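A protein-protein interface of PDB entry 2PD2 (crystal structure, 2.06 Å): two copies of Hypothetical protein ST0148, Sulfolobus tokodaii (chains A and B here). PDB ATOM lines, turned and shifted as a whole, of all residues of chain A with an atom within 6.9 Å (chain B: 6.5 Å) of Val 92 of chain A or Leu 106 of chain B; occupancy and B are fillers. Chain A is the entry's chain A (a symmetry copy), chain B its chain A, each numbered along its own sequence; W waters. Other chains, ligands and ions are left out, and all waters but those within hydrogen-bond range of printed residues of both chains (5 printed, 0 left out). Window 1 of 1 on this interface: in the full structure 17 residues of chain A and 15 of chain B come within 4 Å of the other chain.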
ATOM      1  N   GLN A   6       0.873  -8.848  -4.753  1.00  0.00           N
ATOM      2  CA  GLN A   6       2.097  -9.320  -4.114  1.00  0.00           C
ATOM      3  C   GLN A   6       1.982 -10.787  -3.706  1.00  0.00           C
ATOM      4  O   GLN A   6       0.953 -11.210  -3.190  1.00  0.00           O
ATOM      5  CB  GLN A   6       2.395  -8.497  -2.858  1.00  0.00           C
ATOM      6  CG  GLN A   6       3.457  -9.125  -1.942  1.00  0.00           C
ATOM      7  CD  GLN A   6       3.406  -8.563  -0.535  1.00  0.00           C
ATOM      8  OE1 GLN A   6       2.324  -8.333   0.009  1.00  0.00           O
ATOM      9  NE2 GLN A   6       4.573  -8.354   0.068  1.00  0.00           N
ATOM     10  N   LYS A   8       4.598 -13.564  -1.724  1.00  0.00           N
ATOM     11  CA  LYS A   8       5.907 -13.721  -1.094  1.00  0.00           C
ATOM     12  C   LYS A   8       6.218 -15.111  -0.543  1.00  0.00           C
ATOM     13  O   LYS A   8       7.384 -15.462  -0.364  1.00  0.00           O
ATOM     14  CB  LYS A   8       6.058 -12.697   0.037  1.00  0.00           C
ATOM     15  CG  LYS A   8       4.931 -12.736   1.073  1.00  0.00           C
ATOM     16  CD  LYS A   8       5.200 -11.788   2.248  1.00  0.00           C
ATOM     17  CE  LYS A   8       3.997 -11.668   3.190  1.00  0.00           C
ATOM     18  NZ  LYS A   8       2.895 -10.801   2.644  1.00  0.00           N
ATOM     19  N   VAL A  35       3.820  -9.172  -8.548  1.00  0.00           N
ATOM     20  CA  VAL A  35       5.204  -9.096  -8.087  1.00  0.00           C
ATOM     21  C   VAL A  35       5.525 -10.236  -7.119  1.00  0.00           C
ATOM     22  O   VAL A  35       4.939 -10.324  -6.034  1.00  0.00           O
ATOM     23  CB  VAL A  35       5.465  -7.763  -7.351  1.00  0.00           C
ATOM     24  CG1 VAL A  35       6.895  -7.741  -6.792  1.00  0.00           C
ATOM     25  CG2 VAL A  35       5.228  -6.591  -8.295  1.00  0.00           C
ATOM     26  N   HIS A  37       8.263 -12.040  -4.664  1.00  0.00           N
ATOM     27  CA  HIS A  37       9.511 -11.836  -3.952  1.00  0.00           C
ATOM     28  C   HIS A  37       9.676 -12.826  -2.809  1.00  0.00           C
ATOM     29  O   HIS A  37       8.816 -13.692  -2.590  1.00  0.00           O
ATOM     30  CB  HIS A  37       9.660 -10.379  -3.471  1.00  0.00           C
ATOM     31  CG  HIS A  37       8.661  -9.952  -2.438  1.00  0.00           C
ATOM     32  ND1 HIS A  37       9.033  -9.554  -1.174  1.00  0.00           N
ATOM     33  CD2 HIS A  37       7.317  -9.790  -2.504  1.00  0.00           C
ATOM     34  CE1 HIS A  37       7.964  -9.167  -0.501  1.00  0.00           C
ATOM     35  NE2 HIS A  37       6.911  -9.296  -1.288  1.00  0.00           N
ATOM     36  N   GLN A  38      10.783 -12.704  -2.084  1.00  0.00           N
ATOM     37  CA  GLN A  38      11.104 -13.649  -1.019  1.00  0.00           C
ATOM     38  C   GLN A  38      11.108 -15.049  -1.659  1.00  0.00           C
ATOM     39  O   GLN A  38      11.486 -15.191  -2.816  1.00  0.00           O
ATOM     40  CB  GLN A  38      10.094 -13.581   0.129  1.00  0.00           C
ATOM     41  CG  GLN A  38      10.101 -12.260   0.896  1.00  0.00           C
ATOM     42  CD  GLN A  38       9.369 -12.350   2.229  1.00  0.00           C
ATOM     43  OE1 GLN A  38       8.658 -13.321   2.498  1.00  0.00           O
ATOM     44  NE2 GLN A  38       9.540 -11.331   3.071  1.00  0.00           N
ATOM     45  N   CYS A  67      11.429 -10.318  -8.241  1.00  0.00           N
ATOM     46  CA  CYS A  67      12.341  -9.475  -7.467  1.00  0.00           C
ATOM     47  C   CYS A  67      13.804  -9.904  -7.605  1.00  0.00           C
ATOM     48  O   CYS A  67      14.149 -11.049  -7.317  1.00  0.00           O
ATOM     49  CB  CYS A  67      11.939  -9.506  -5.987  1.00  0.00           C
ATOM     50  SG  CYS A  67      13.158  -8.773  -4.864  1.00  0.00           S
ATOM     51  N   ASN A  69      16.423  -8.908  -5.816  1.00  0.00           N
ATOM     52  CA  ASN A  69      17.005  -9.218  -4.511  1.00  0.00           C
ATOM     53  C   ASN A  69      16.690 -10.655  -4.130  1.00  0.00           C
ATOM     54  O   ASN A  69      17.541 -11.374  -3.603  1.00  0.00           O
ATOM     55  CB  ASN A  69      16.462  -8.290  -3.419  1.00  0.00           C
ATOM     56  CG  ASN A  69      17.033  -6.892  -3.505  1.00  0.00           C
ATOM     57  OD1 ASN A  69      18.229  -6.710  -3.753  1.00  0.00           O
ATOM     58  ND2 ASN A  69      16.188  -5.893  -3.282  1.00  0.00           N
ATOM     59  N   VAL A  88      12.583  -6.530 -11.420  1.00  0.00           N
ATOM     60  CA  VAL A  88      12.766  -5.201 -10.851  1.00  0.00           C
ATOM     61  C   VAL A  88      13.859  -5.322  -9.802  1.00  0.00           C
ATOM     62  O   VAL A  88      14.108  -6.412  -9.281  1.00  0.00           O
ATOM     63  CB  VAL A  88      11.471  -4.647 -10.197  1.00  0.00           C
ATOM     64  CG1 VAL A  88      10.417  -4.431 -11.263  1.00  0.00           C
ATOM     65  CG2 VAL A  88      10.966  -5.598  -9.111  1.00  0.00           C
ATOM     66  N   THR A  89      14.524  -4.211  -9.506  1.00  0.00           N
ATOM     67  CA  THR A  89      15.608  -4.220  -8.532  1.00  0.00           C
ATOM     68  C   THR A  89      15.129  -4.692  -7.164  1.00  0.00           C
ATOM     69  O   THR A  89      15.829  -5.436  -6.471  1.00  0.00           O
ATOM     70  CB  THR A  89      16.245  -2.810  -8.387  1.00  0.00           C
ATOM     71  OG1 THR A  89      15.267  -1.888  -7.894  1.00  0.00           O
ATOM     72  CG2 THR A  89      16.754  -2.310  -9.732  1.00  0.00           C
ATOM     73  N   SER A  90      13.929  -4.263  -6.788  1.00  0.00           N
ATOM     74  CA  SER A  90      13.341  -4.623  -5.505  1.00  0.00           C
ATOM     75  C   SER A  90      11.850  -4.883  -5.666  1.00  0.00           C
ATOM     76  O   SER A  90      11.119  -4.047  -6.197  1.00  0.00           O
ATOM     77  CB  SER A  90      13.566  -3.486  -4.502  1.00  0.00           C
ATOM     78  OG  SER A  90      12.822  -3.675  -3.316  1.00  0.00           O
ATOM     79  N   GLY A  91      11.406  -6.050  -5.219  1.00  0.00           N
ATOM     80  CA  GLY A  91      10.000  -6.388  -5.320  1.00  0.00           C
ATOM     81  C   GLY A  91       9.165  -5.474  -4.450  1.00  0.00           C
ATOM     82  O   GLY A  91       8.112  -4.996  -4.873  1.00  0.00           O
ATOM     83  N   VAL A  92       9.640  -5.222  -3.235  1.00  0.00           N
ATOM     84  CA  VAL A  92       8.923  -4.357  -2.309  1.00  0.00           C
ATOM     85  C   VAL A  92       8.953  -2.909  -2.793  1.00  0.00           C
ATOM     86  O   VAL A  92       7.991  -2.173  -2.607  1.00  0.00           O
ATOM     87  CB  VAL A  92       9.505  -4.470  -0.878  1.00  0.00           C
ATOM     88  CG1 VAL A  92       9.260  -5.876  -0.347  1.00  0.00           C
ATOM     89  CG2 VAL A  92      10.998  -4.170  -0.880  1.00  0.00           C
ATOM     90  N   GLY A  93      10.051  -2.505  -3.424  1.00  0.00           N
ATOM     91  CA  GLY A  93      10.132  -1.151  -3.947  1.00  0.00           C
ATOM     92  C   GLY A  93       9.122  -0.958  -5.072  1.00  0.00           C
ATOM     93  O   GLY A  93       8.509   0.102  -5.201  1.00  0.00           O
ATOM     94  N   GLU A  94       8.951  -1.992  -5.892  1.00  0.00           N
ATOM     95  CA  GLU A  94       8.002  -1.952  -7.001  1.00  0.00           C
ATOM     96  C   GLU A  94       6.573  -1.869  -6.456  1.00  0.00           C
ATOM     97  O   GLU A  94       5.756  -1.068  -6.921  1.00  0.00           O
ATOM     98  CB  GLU A  94       8.157  -3.214  -7.860  1.00  0.00           C
ATOM     99  CG  GLU A  94       7.115  -3.371  -8.969  1.00  0.00           C
ATOM    100  CD  GLU A  94       7.305  -2.391 -10.116  1.00  0.00           C
ATOM    101  OE1 GLU A  94       8.164  -1.494 -10.002  1.00  0.00           O
ATOM    102  OE2 GLU A  94       6.589  -2.516 -11.133  1.00  0.00           O
ATOM    103  N   ILE A  95       6.279  -2.703  -5.464  1.00  0.00           N
ATOM    104  CA  ILE A  95       4.956  -2.741  -4.850  1.00  0.00           C
ATOM    105  C   ILE A  95       4.596  -1.366  -4.289  1.00  0.00           C
ATOM    106  O   ILE A  95       3.494  -0.857  -4.508  1.00  0.00           O
ATOM    107  CB  ILE A  95       4.919  -3.823  -3.736  1.00  0.00           C
ATOM    108  CG1 ILE A  95       4.966  -5.218  -4.380  1.00  0.00           C
ATOM    109  CG2 ILE A  95       3.674  -3.664  -2.878  1.00  0.00           C
ATOM    110  CD1 ILE A  95       5.215  -6.363  -3.397  1.00  0.00           C
ATOM    111  N   VAL A  96       5.540  -0.749  -3.587  1.00  0.00           N
ATOM    112  CA  VAL A  96       5.301   0.572  -3.022  1.00  0.00           C
ATOM    113  C   VAL A  96       5.145   1.629  -4.123  1.00  0.00           C
ATOM    114  O   VAL A  96       4.231   2.450  -4.077  1.00  0.00           O
ATOM    115  CB  VAL A  96       6.448   0.966  -2.052  1.00  0.00           C
ATOM    116  CG1 VAL A  96       6.362   2.446  -1.704  1.00  0.00           C
ATOM    117  CG2 VAL A  96       6.352   0.113  -0.768  1.00  0.00           C
ATOM    118  N   ARG A  97       6.030   1.608  -5.117  1.00  0.00           N
ATOM    119  CA  ARG A  97       5.952   2.588  -6.202  1.00  0.00           C
ATOM    120  C   ARG A  97       4.654   2.490  -7.000  1.00  0.00           C
ATOM    121  O   ARG A  97       4.040   3.509  -7.303  1.00  0.00           O
ATOM    122  CB  ARG A  97       7.155   2.458  -7.150  1.00  0.00           C
ATOM    123  CG  ARG A  97       8.411   3.171  -6.661  1.00  0.00           C
ATOM    124  CD  ARG A  97       9.509   3.173  -7.720  1.00  0.00           C
ATOM    125  NE  ARG A  97      10.120   1.858  -7.879  1.00  0.00           N
ATOM    126  CZ  ARG A  97      11.144   1.418  -7.151  1.00  0.00           C
ATOM    127  NH1 ARG A  97      11.676   2.195  -6.217  1.00  0.00           N
ATOM    128  NH2 ARG A  97      11.632   0.201  -7.352  1.00  0.00           N
ATOM    129  N   GLN A  99       1.824   1.442  -5.980  1.00  0.00           N
ATOM    130  CA  GLN A  99       0.751   1.981  -5.149  1.00  0.00           C
ATOM    131  C   GLN A  99       0.753   3.505  -5.167  1.00  0.00           C
ATOM    132  O   GLN A  99      -0.305   4.126  -5.208  1.00  0.00           O
ATOM    133  CB  GLN A  99       0.871   1.499  -3.702  1.00  0.00           C
ATOM    134  CG  GLN A  99       0.445   0.056  -3.477  1.00  0.00           C
ATOM    135  CD  GLN A  99       0.389  -0.292  -1.999  1.00  0.00           C
ATOM    136  OE1 GLN A  99      -0.510   0.140  -1.283  1.00  0.00           O
ATOM    137  NE2 GLN A  99       1.365  -1.065  -1.537  1.00  0.00           N
ATOM    138  N   TYR A 105      -3.413  -2.260  -4.163  1.00  0.00           N
ATOM    139  CA  TYR A 105      -2.620  -3.330  -3.569  1.00  0.00           C
ATOM    140  C   TYR A 105      -3.427  -4.540  -3.106  1.00  0.00           C
ATOM    141  O   TYR A 105      -4.464  -4.401  -2.452  1.00  0.00           O
ATOM    142  CB  TYR A 105      -1.832  -2.721  -2.402  1.00  0.00           C
ATOM    143  CG  TYR A 105      -1.011  -3.661  -1.549  1.00  0.00           C
ATOM    144  CD1 TYR A 105      -0.239  -4.676  -2.112  1.00  0.00           C
ATOM    145  CD2 TYR A 105      -0.947  -3.475  -0.170  1.00  0.00           C
ATOM    146  CE1 TYR A 105       0.586  -5.477  -1.310  1.00  0.00           C
ATOM    147  CE2 TYR A 105      -0.133  -4.258   0.632  1.00  0.00           C
ATOM    148  CZ  TYR A 105       0.630  -5.256   0.060  1.00  0.00           C
ATOM    149  OH  TYR A 105       1.450  -5.998   0.868  1.00  0.00           O
ATOM    150  N   VAL B   3       6.096   4.910   3.967  1.00  0.00           N
ATOM    151  CA  VAL B   3       5.652   3.520   3.910  1.00  0.00           C
ATOM    152  C   VAL B   3       5.403   2.954   5.307  1.00  0.00           C
ATOM    153  O   VAL B   3       6.269   3.033   6.176  1.00  0.00           O
ATOM    154  CB  VAL B   3       6.717   2.620   3.233  1.00  0.00           C
ATOM    155  CG1 VAL B   3       6.176   1.204   3.062  1.00  0.00           C
ATOM    156  CG2 VAL B   3       7.125   3.210   1.882  1.00  0.00           C
ATOM    157  N   VAL B   4       4.211   2.412   5.529  1.00  0.00           N
ATOM    158  CA  VAL B   4       3.912   1.795   6.807  1.00  0.00           C
ATOM    159  C   VAL B   4       3.974   0.288   6.532  1.00  0.00           C
ATOM    160  O   VAL B   4       3.208  -0.253   5.729  1.00  0.00           O
ATOM    161  CB  VAL B   4       2.519   2.236   7.358  1.00  0.00           C
ATOM    162  CG1 VAL B   4       1.409   1.856   6.400  1.00  0.00           C
ATOM    163  CG2 VAL B   4       2.292   1.622   8.728  1.00  0.00           C
ATOM    164  N   VAL B   5       4.933  -0.369   7.171  1.00  0.00           N
ATOM    165  CA  VAL B   5       5.155  -1.799   7.003  1.00  0.00           C
ATOM    166  C   VAL B   5       4.547  -2.630   8.129  1.00  0.00           C
ATOM    167  O   VAL B   5       4.727  -2.330   9.304  1.00  0.00           O
ATOM    168  CB  VAL B   5       6.661  -2.114   6.966  1.00  0.00           C
ATOM    169  CG1 VAL B   5       6.877  -3.622   6.792  1.00  0.00           C
ATOM    170  CG2 VAL B   5       7.336  -1.335   5.842  1.00  0.00           C
ATOM    171  N   GLN B   6       3.844  -3.693   7.760  1.00  0.00           N
ATOM    172  CA  GLN B   6       3.231  -4.573   8.749  1.00  0.00           C
ATOM    173  C   GLN B   6       3.930  -5.930   8.796  1.00  0.00           C
ATOM    174  O   GLN B   6       4.262  -6.495   7.759  1.00  0.00           O
ATOM    175  CB  GLN B   6       1.756  -4.808   8.413  1.00  0.00           C
ATOM    176  CG  GLN B   6       1.120  -5.973   9.187  1.00  0.00           C
ATOM    177  CD  GLN B   6      -0.152  -6.472   8.531  1.00  0.00           C
ATOM    178  OE1 GLN B   6      -0.231  -6.562   7.304  1.00  0.00           O
ATOM    179  NE2 GLN B   6      -1.149  -6.814   9.342  1.00  0.00           N
ATOM    180  N   ILE B   7       4.161  -6.435  10.003  1.00  0.00           N
ATOM    181  CA  ILE B   7       4.754  -7.759  10.192  1.00  0.00           C
ATOM    182  C   ILE B   7       3.936  -8.391  11.314  1.00  0.00           C
ATOM    183  O   ILE B   7       3.856  -7.833  12.408  1.00  0.00           O
ATOM    184  CB  ILE B   7       6.234  -7.697  10.627  1.00  0.00           C
ATOM    185  CG1 ILE B   7       7.054  -6.890   9.619  1.00  0.00           C
ATOM    186  CG2 ILE B   7       6.794  -9.108  10.713  1.00  0.00           C
ATOM    187  CD1 ILE B   7       8.533  -6.798   9.970  1.00  0.00           C
ATOM    188  N   SER B  19      13.435  -7.848   3.950  1.00  0.00           N
ATOM    189  CA  SER B  19      12.639  -7.130   2.962  1.00  0.00           C
ATOM    190  C   SER B  19      12.606  -5.636   3.281  1.00  0.00           C
ATOM    191  O   SER B  19      12.628  -4.802   2.379  1.00  0.00           O
ATOM    192  CB  SER B  19      11.220  -7.697   2.910  1.00  0.00           C
ATOM    193  OG  SER B  19      11.205  -8.965   2.275  1.00  0.00           O
ATOM    194  N   VAL B  20      12.550  -5.292   4.564  1.00  0.00           N
ATOM    195  CA  VAL B  20      12.555  -3.883   4.950  1.00  0.00           C
ATOM    196  C   VAL B  20      13.910  -3.278   4.574  1.00  0.00           C
ATOM    197  O   VAL B  20      13.988  -2.144   4.096  1.00  0.00           O
ATOM    198  CB  VAL B  20      12.306  -3.712   6.463  1.00  0.00           C
ATOM    199  CG1 VAL B  20      12.482  -2.248   6.853  1.00  0.00           C
ATOM    200  CG2 VAL B  20      10.887  -4.163   6.803  1.00  0.00           C
ATOM    201  N   ASN B  22      15.704  -4.239   2.158  1.00  0.00           N
ATOM    202  CA  ASN B  22      15.637  -4.100   0.704  1.00  0.00           C
ATOM    203  C   ASN B  22      14.877  -2.829   0.325  1.00  0.00           C
ATOM    204  O   ASN B  22      15.280  -2.112  -0.586  1.00  0.00           O
ATOM    205  CB  ASN B  22      14.968  -5.328   0.062  1.00  0.00           C
ATOM    206  CG  ASN B  22      15.869  -6.566   0.071  1.00  0.00           C
ATOM    207  OD1 ASN B  22      17.088  -6.457   0.220  1.00  0.00           O
ATOM    208  ND2 ASN B  22      15.270  -7.745  -0.105  1.00  0.00           N
ATOM    209  N   LEU B  23      13.776  -2.560   1.022  1.00  0.00           N
ATOM    210  CA  LEU B  23      12.977  -1.364   0.765  1.00  0.00           C
ATOM    211  C   LEU B  23      13.852  -0.129   0.955  1.00  0.00           C
ATOM    212  O   LEU B  23      13.941   0.732   0.079  1.00  0.00           O
ATOM    213  CB  LEU B  23      11.790  -1.295   1.736  1.00  0.00           C
ATOM    214  CG  LEU B  23      10.886  -0.065   1.602  1.00  0.00           C
ATOM    215  CD1 LEU B  23      10.269  -0.048   0.213  1.00  0.00           C
ATOM    216  CD2 LEU B  23       9.796  -0.095   2.664  1.00  0.00           C
ATOM    217  N   TYR B  24      14.488  -0.055   2.121  1.00  0.00           N
ATOM    218  CA  TYR B  24      15.374   1.054   2.466  1.00  0.00           C
ATOM    219  C   TYR B  24      16.412   1.300   1.374  1.00  0.00           C
ATOM    220  O   TYR B  24      16.625   2.436   0.944  1.00  0.00           O
ATOM    221  CB  TYR B  24      16.093   0.747   3.782  1.00  0.00           C
ATOM    222  CG  TYR B  24      17.147   1.763   4.166  1.00  0.00           C
ATOM    223  CD1 TYR B  24      16.804   2.930   4.849  1.00  0.00           C
ATOM    224  CD2 TYR B  24      18.489   1.556   3.844  1.00  0.00           C
ATOM    225  CE1 TYR B  24      17.770   3.865   5.204  1.00  0.00           C
ATOM    226  CE2 TYR B  24      19.462   2.483   4.193  1.00  0.00           C
ATOM    227  CZ  TYR B  24      19.096   3.634   4.872  1.00  0.00           C
ATOM    228  OH  TYR B  24      20.057   4.553   5.211  1.00  0.00           O
ATOM    229  N   ASP B  26      16.262   0.427  -1.720  1.00  0.00           N
ATOM    230  CA  ASP B  26      15.674   0.691  -3.025  1.00  0.00           C
ATOM    231  C   ASP B  26      14.965   2.024  -3.211  1.00  0.00           C
ATOM    232  O   ASP B  26      14.932   2.556  -4.319  1.00  0.00           O
ATOM    233  CB  ASP B  26      14.715  -0.443  -3.390  1.00  0.00           C
ATOM    234  CG  ASP B  26      14.393  -0.474  -4.872  1.00  0.00           C
ATOM    235  OD1 ASP B  26      15.339  -0.616  -5.675  1.00  0.00           O
ATOM    236  OD2 ASP B  26      13.204  -0.355  -5.235  1.00  0.00           O
ATOM    237  N   ILE B  27      14.392   2.566  -2.143  1.00  0.00           N
ATOM    238  CA  ILE B  27      13.679   3.831  -2.246  1.00  0.00           C
ATOM    239  C   ILE B  27      14.420   4.966  -1.553  1.00  0.00           C
ATOM    240  O   ILE B  27      14.479   5.029  -0.327  1.00  0.00           O
ATOM    241  CB  ILE B  27      12.249   3.711  -1.664  1.00  0.00           C
ATOM    242  CG1 ILE B  27      11.468   2.647  -2.451  1.00  0.00           C
ATOM    243  CG2 ILE B  27      11.526   5.047  -1.772  1.00  0.00           C
ATOM    244  CD1 ILE B  27      10.021   2.502  -2.031  1.00  0.00           C
ATOM    245  N   ILE B 104       1.958   4.566   2.439  1.00  0.00           N
ATOM    246  CA  ILE B 104       1.775   3.400   1.592  1.00  0.00           C
ATOM    247  C   ILE B 104       1.969   2.122   2.415  1.00  0.00           C
ATOM    248  O   ILE B 104       2.964   1.951   3.115  1.00  0.00           O
ATOM    249  CB  ILE B 104       2.756   3.429   0.402  1.00  0.00           C
ATOM    250  CG1 ILE B 104       2.428   4.637  -0.489  1.00  0.00           C
ATOM    251  CG2 ILE B 104       2.657   2.122  -0.399  1.00  0.00           C
ATOM    252  CD1 ILE B 104       3.437   4.904  -1.584  1.00  0.00           C
ATOM    253  N   TYR B 105       0.993   1.232   2.307  1.00  0.00           N
ATOM    254  CA  TYR B 105       0.957  -0.030   3.038  1.00  0.00           C
ATOM    255  C   TYR B 105       1.732  -1.169   2.382  1.00  0.00           C
ATOM    256  O   TYR B 105       1.620  -1.403   1.175  1.00  0.00           O
ATOM    257  CB  TYR B 105      -0.517  -0.409   3.224  1.00  0.00           C
ATOM    258  CG  TYR B 105      -0.818  -1.746   3.863  1.00  0.00           C
ATOM    259  CD1 TYR B 105      -0.108  -2.204   4.972  1.00  0.00           C
ATOM    260  CD2 TYR B 105      -1.881  -2.518   3.398  1.00  0.00           C
ATOM    261  CE1 TYR B 105      -0.465  -3.403   5.605  1.00  0.00           C
ATOM    262  CE2 TYR B 105      -2.244  -3.703   4.017  1.00  0.00           C
ATOM    263  CZ  TYR B 105      -1.535  -4.141   5.117  1.00  0.00           C
ATOM    264  OH  TYR B 105      -1.931  -5.300   5.731  1.00  0.00           O
ATOM    265  N   LEU B 106       2.518  -1.871   3.194  1.00  0.00           N
ATOM    266  CA  LEU B 106       3.307  -3.010   2.735  1.00  0.00           C
ATOM    267  C   LEU B 106       3.189  -4.115   3.780  1.00  0.00           C
ATOM    268  O   LEU B 106       3.649  -3.957   4.918  1.00  0.00           O
ATOM    269  CB  LEU B 106       4.783  -2.621   2.557  1.00  0.00           C
ATOM    270  CG  LEU B 106       5.723  -3.780   2.192  1.00  0.00           C
ATOM    271  CD1 LEU B 106       5.299  -4.389   0.851  1.00  0.00           C
ATOM    272  CD2 LEU B 106       7.154  -3.282   2.116  1.00  0.00           C
ATOM    273  N   ALA B 107       2.560  -5.225   3.402  1.00  0.00           N
ATOM    274  CA  ALA B 107       2.386  -6.347   4.324  1.00  0.00           C
ATOM    275  C   ALA B 107       3.500  -7.372   4.140  1.00  0.00           C
ATOM    276  O   ALA B 107       3.693  -7.901   3.044  1.00  0.00           O
ATOM    277  CB  ALA B 107       1.031  -7.006   4.097  1.00  0.00           C
ATOM    278  N   LEU B 108       4.238  -7.637   5.211  1.00  0.00           N
ATOM    279  CA  LEU B 108       5.327  -8.604   5.171  1.00  0.00           C
ATOM    280  C   LEU B 108       5.084  -9.726   6.175  1.00  0.00           C
ATOM    281  O   LEU B 108       3.963  -9.786   6.723  1.00  0.00           O
ATOM    282  CB  LEU B 108       6.662  -7.918   5.469  1.00  0.00           C
ATOM    283  CG  LEU B 108       7.154  -6.911   4.423  1.00  0.00           C
ATOM    284  CD1 LEU B 108       8.415  -6.223   4.928  1.00  0.00           C
ATOM    285  CD2 LEU B 108       7.426  -7.627   3.105  1.00  0.00           C
ATOM    286  OXT LEU B 108       6.012 -10.538   6.389  1.00  0.00           O
HETATM  287  O   HOH W   1      16.896  -3.319  -2.487  1.00  0.00           O
HETATM  288  O   HOH W   2      -1.380   1.797   0.523  1.00  0.00           O
HETATM  289  O   HOH W   3       8.057 -11.861   5.563  1.00  0.00           O
HETATM  290  O   HOH W   4      16.696 -10.541  -0.383  1.00  0.00           O
HETATM  291  O   HOH W   5      12.194  -9.181  -0.438  1.00  0.00           O
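Water W3 lies within hydrogen-bond range of the chain-end carboxylate of Leu 108 of chain B (2.6 Å) and the side-chain amide nitrogen of Gln 38 of chain A (2.9 Å).
Water W2 bridges OE1 of Gln 99 of chain A (2.6 Å) and N of Tyr 105 of chain B (3.0 Å).
Water W1 lies within hydrogen-bond range of O of Asn 22 of chain B and ND2 of Asn 69 of chain A.
Water W5 lies within hydrogen-bond range of the side-chain hydroxyl of Ser 19 of chain B (2.9 Å), a ring nitrogen (ND1) of His 37 of chain A (3.3 Å) and the side-chain amide nitrogen of Asn 22 of chain B (3.4 Å).
Water W4 lies within hydrogen-bond range of ND2 of Asn 22 of chain B and O of Asn 69 of chain A.
Tyr 105 of chain B touches its own counterpart, Tyr 105 of chain A.
Positions printed for both chains: 6 and 105.
Of the 23 pairs that touch across the chains among the printed residues, 1 has its exchanged pair printed and touching as well.
The backbone NH of Gln 6 of chain B is in hydrogen-bond range of the backbone carbonyl oxygen of Leu 106 of chain B (2.9 Å).
The backbone carbonyl oxygen of Gln 6 of chain B sits at hydrogen-bond distance from the backbone NH of Leu 108 of chain B (2.8 Å).
The side-chain amide nitrogen of Gln 6 of chain A lies within hydrogen-bond range of a ring nitrogen (NE2) of His 37 of chain A, at 2.9 Å.
OE1 of Gln 6 of chain A lies within hydrogen-bond range of OH of Tyr 105 of chain A, at 2.6 Å.
OG of Ser 90 of chain A sits at hydrogen-bond distance from N of Gly 93 of chain A (3.0 Å).
The side-chain hydroxyl (OG) of Ser 19 of chain B sits at hydrogen-bond distance from the side-chain amide nitrogen (NE2) of Gln 38 of chain A (3.0 Å).
The side-chain carboxylate (OD1) of Asp 26 of chain B sits at hydrogen-bond distance from the side-chain hydroxyl (OG1) of Thr 89 of chain A, at 2.6 Å.
The guanidinium group (NH2) of Arg 97 of chain A lies within salt-bridge range of the side-chain carboxylate (OD2) of Asp 26 of chain B, 2.7 Å away.
The side-chain amide nitrogen (NE2) of Gln 99 of chain A is in hydrogen-bond range of the backbone carbonyl oxygen (O) of Tyr 105 of chain B (2.7 Å).
The backbone carbonyl oxygen (O) of Ala 107 of chain B is in hydrogen-bond range of the side-chain amide nitrogen (NE2) of Gln 6 of chain A, 3.1 Å away.
The backbone carbonyl oxygen (O) of Ala 107 of chain B sits at hydrogen-bond distance from the side-chain amino group (NZ) of Lys 8 of chain A (3.0 Å).
The backbone NH (N) of Ala 107 of chain B is in hydrogen-bond range of the side-chain hydroxyl (OH) of Tyr 105 of chain A, at 2.9 Å.
Of the printed residues of chain B, Val 92 of chain A touches Ser 19 (3.7 Å), Leu 23 (3.7 Å) and Leu 106 (3.99 Å).
Printed residues of chain A within 4 Å of Leu 106 of chain B: Val 92 (3.99 Å) and Tyr 105 (3.9 Å).
Printed residues of chain A within 4 Å of Ile 104 of chain B: Val 96 (3.6 Å) and Gln 99 (3.6 Å).
Printed residues of chain B within 4 Å of Lys 8 of chain A: Ala 107 and Leu 108.
Of the printed residues of chain A, Asp 26 of chain B touches Thr 89, Ser 90, Gly 93 and Arg 97.
Cys 67 of chain A touches none of the printed residues of chain B.
The nearest printed residue of chain B that does not touch Val 92 of chain A is Asn 22 of chain B (4.2 Å).
Hydrophobic or aromatic side chains of chain B within 4 Å of the printed part of chain A: Val 3, Leu 23, Ile 27, Ile 104, Tyr 105, Leu 106, Ala 107 and Leu 108.
Of the 19 printed residues of chain A, 13 touch a printed residue of chain B.
Hydrophobic or aromatic side chains of chain A that line the printed part of chain B: His 37, Val 92, Val 96 and Tyr 105.
Among the printed residues, pairs that only touch across the chains: Lys 8 of chain A with Leu 108 of chain B, His 37 of chain A with Leu 108 of chain B, Asn 69 of chain A with Asn 22 of chain B, Ser 90 of chain A with Asn 22 of chain B, Ser 90 of chain A with Asp 26 of chain B, Val 92 of chain A with Ser 19 of chain B, Val 92 of chain A with Leu 23 of chain B, Val 92 of chain A with Leu 106 of chain B, Gly 93 of chain A with Asp 26 of chain B, Val 96 of chain A with Val 3 of chain B, Val 96 of chain A with Ile 27 of chain B, Val 96 of chain A with Ile 104 of chain B, Arg 97 of chain A with Ile 27 of chain B, Gln 99 of chain A with Ile 104 of chain B, Tyr 105 of chain A with Tyr 105 of chain B and Tyr 105 of chain A with Leu 106 of chain B.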
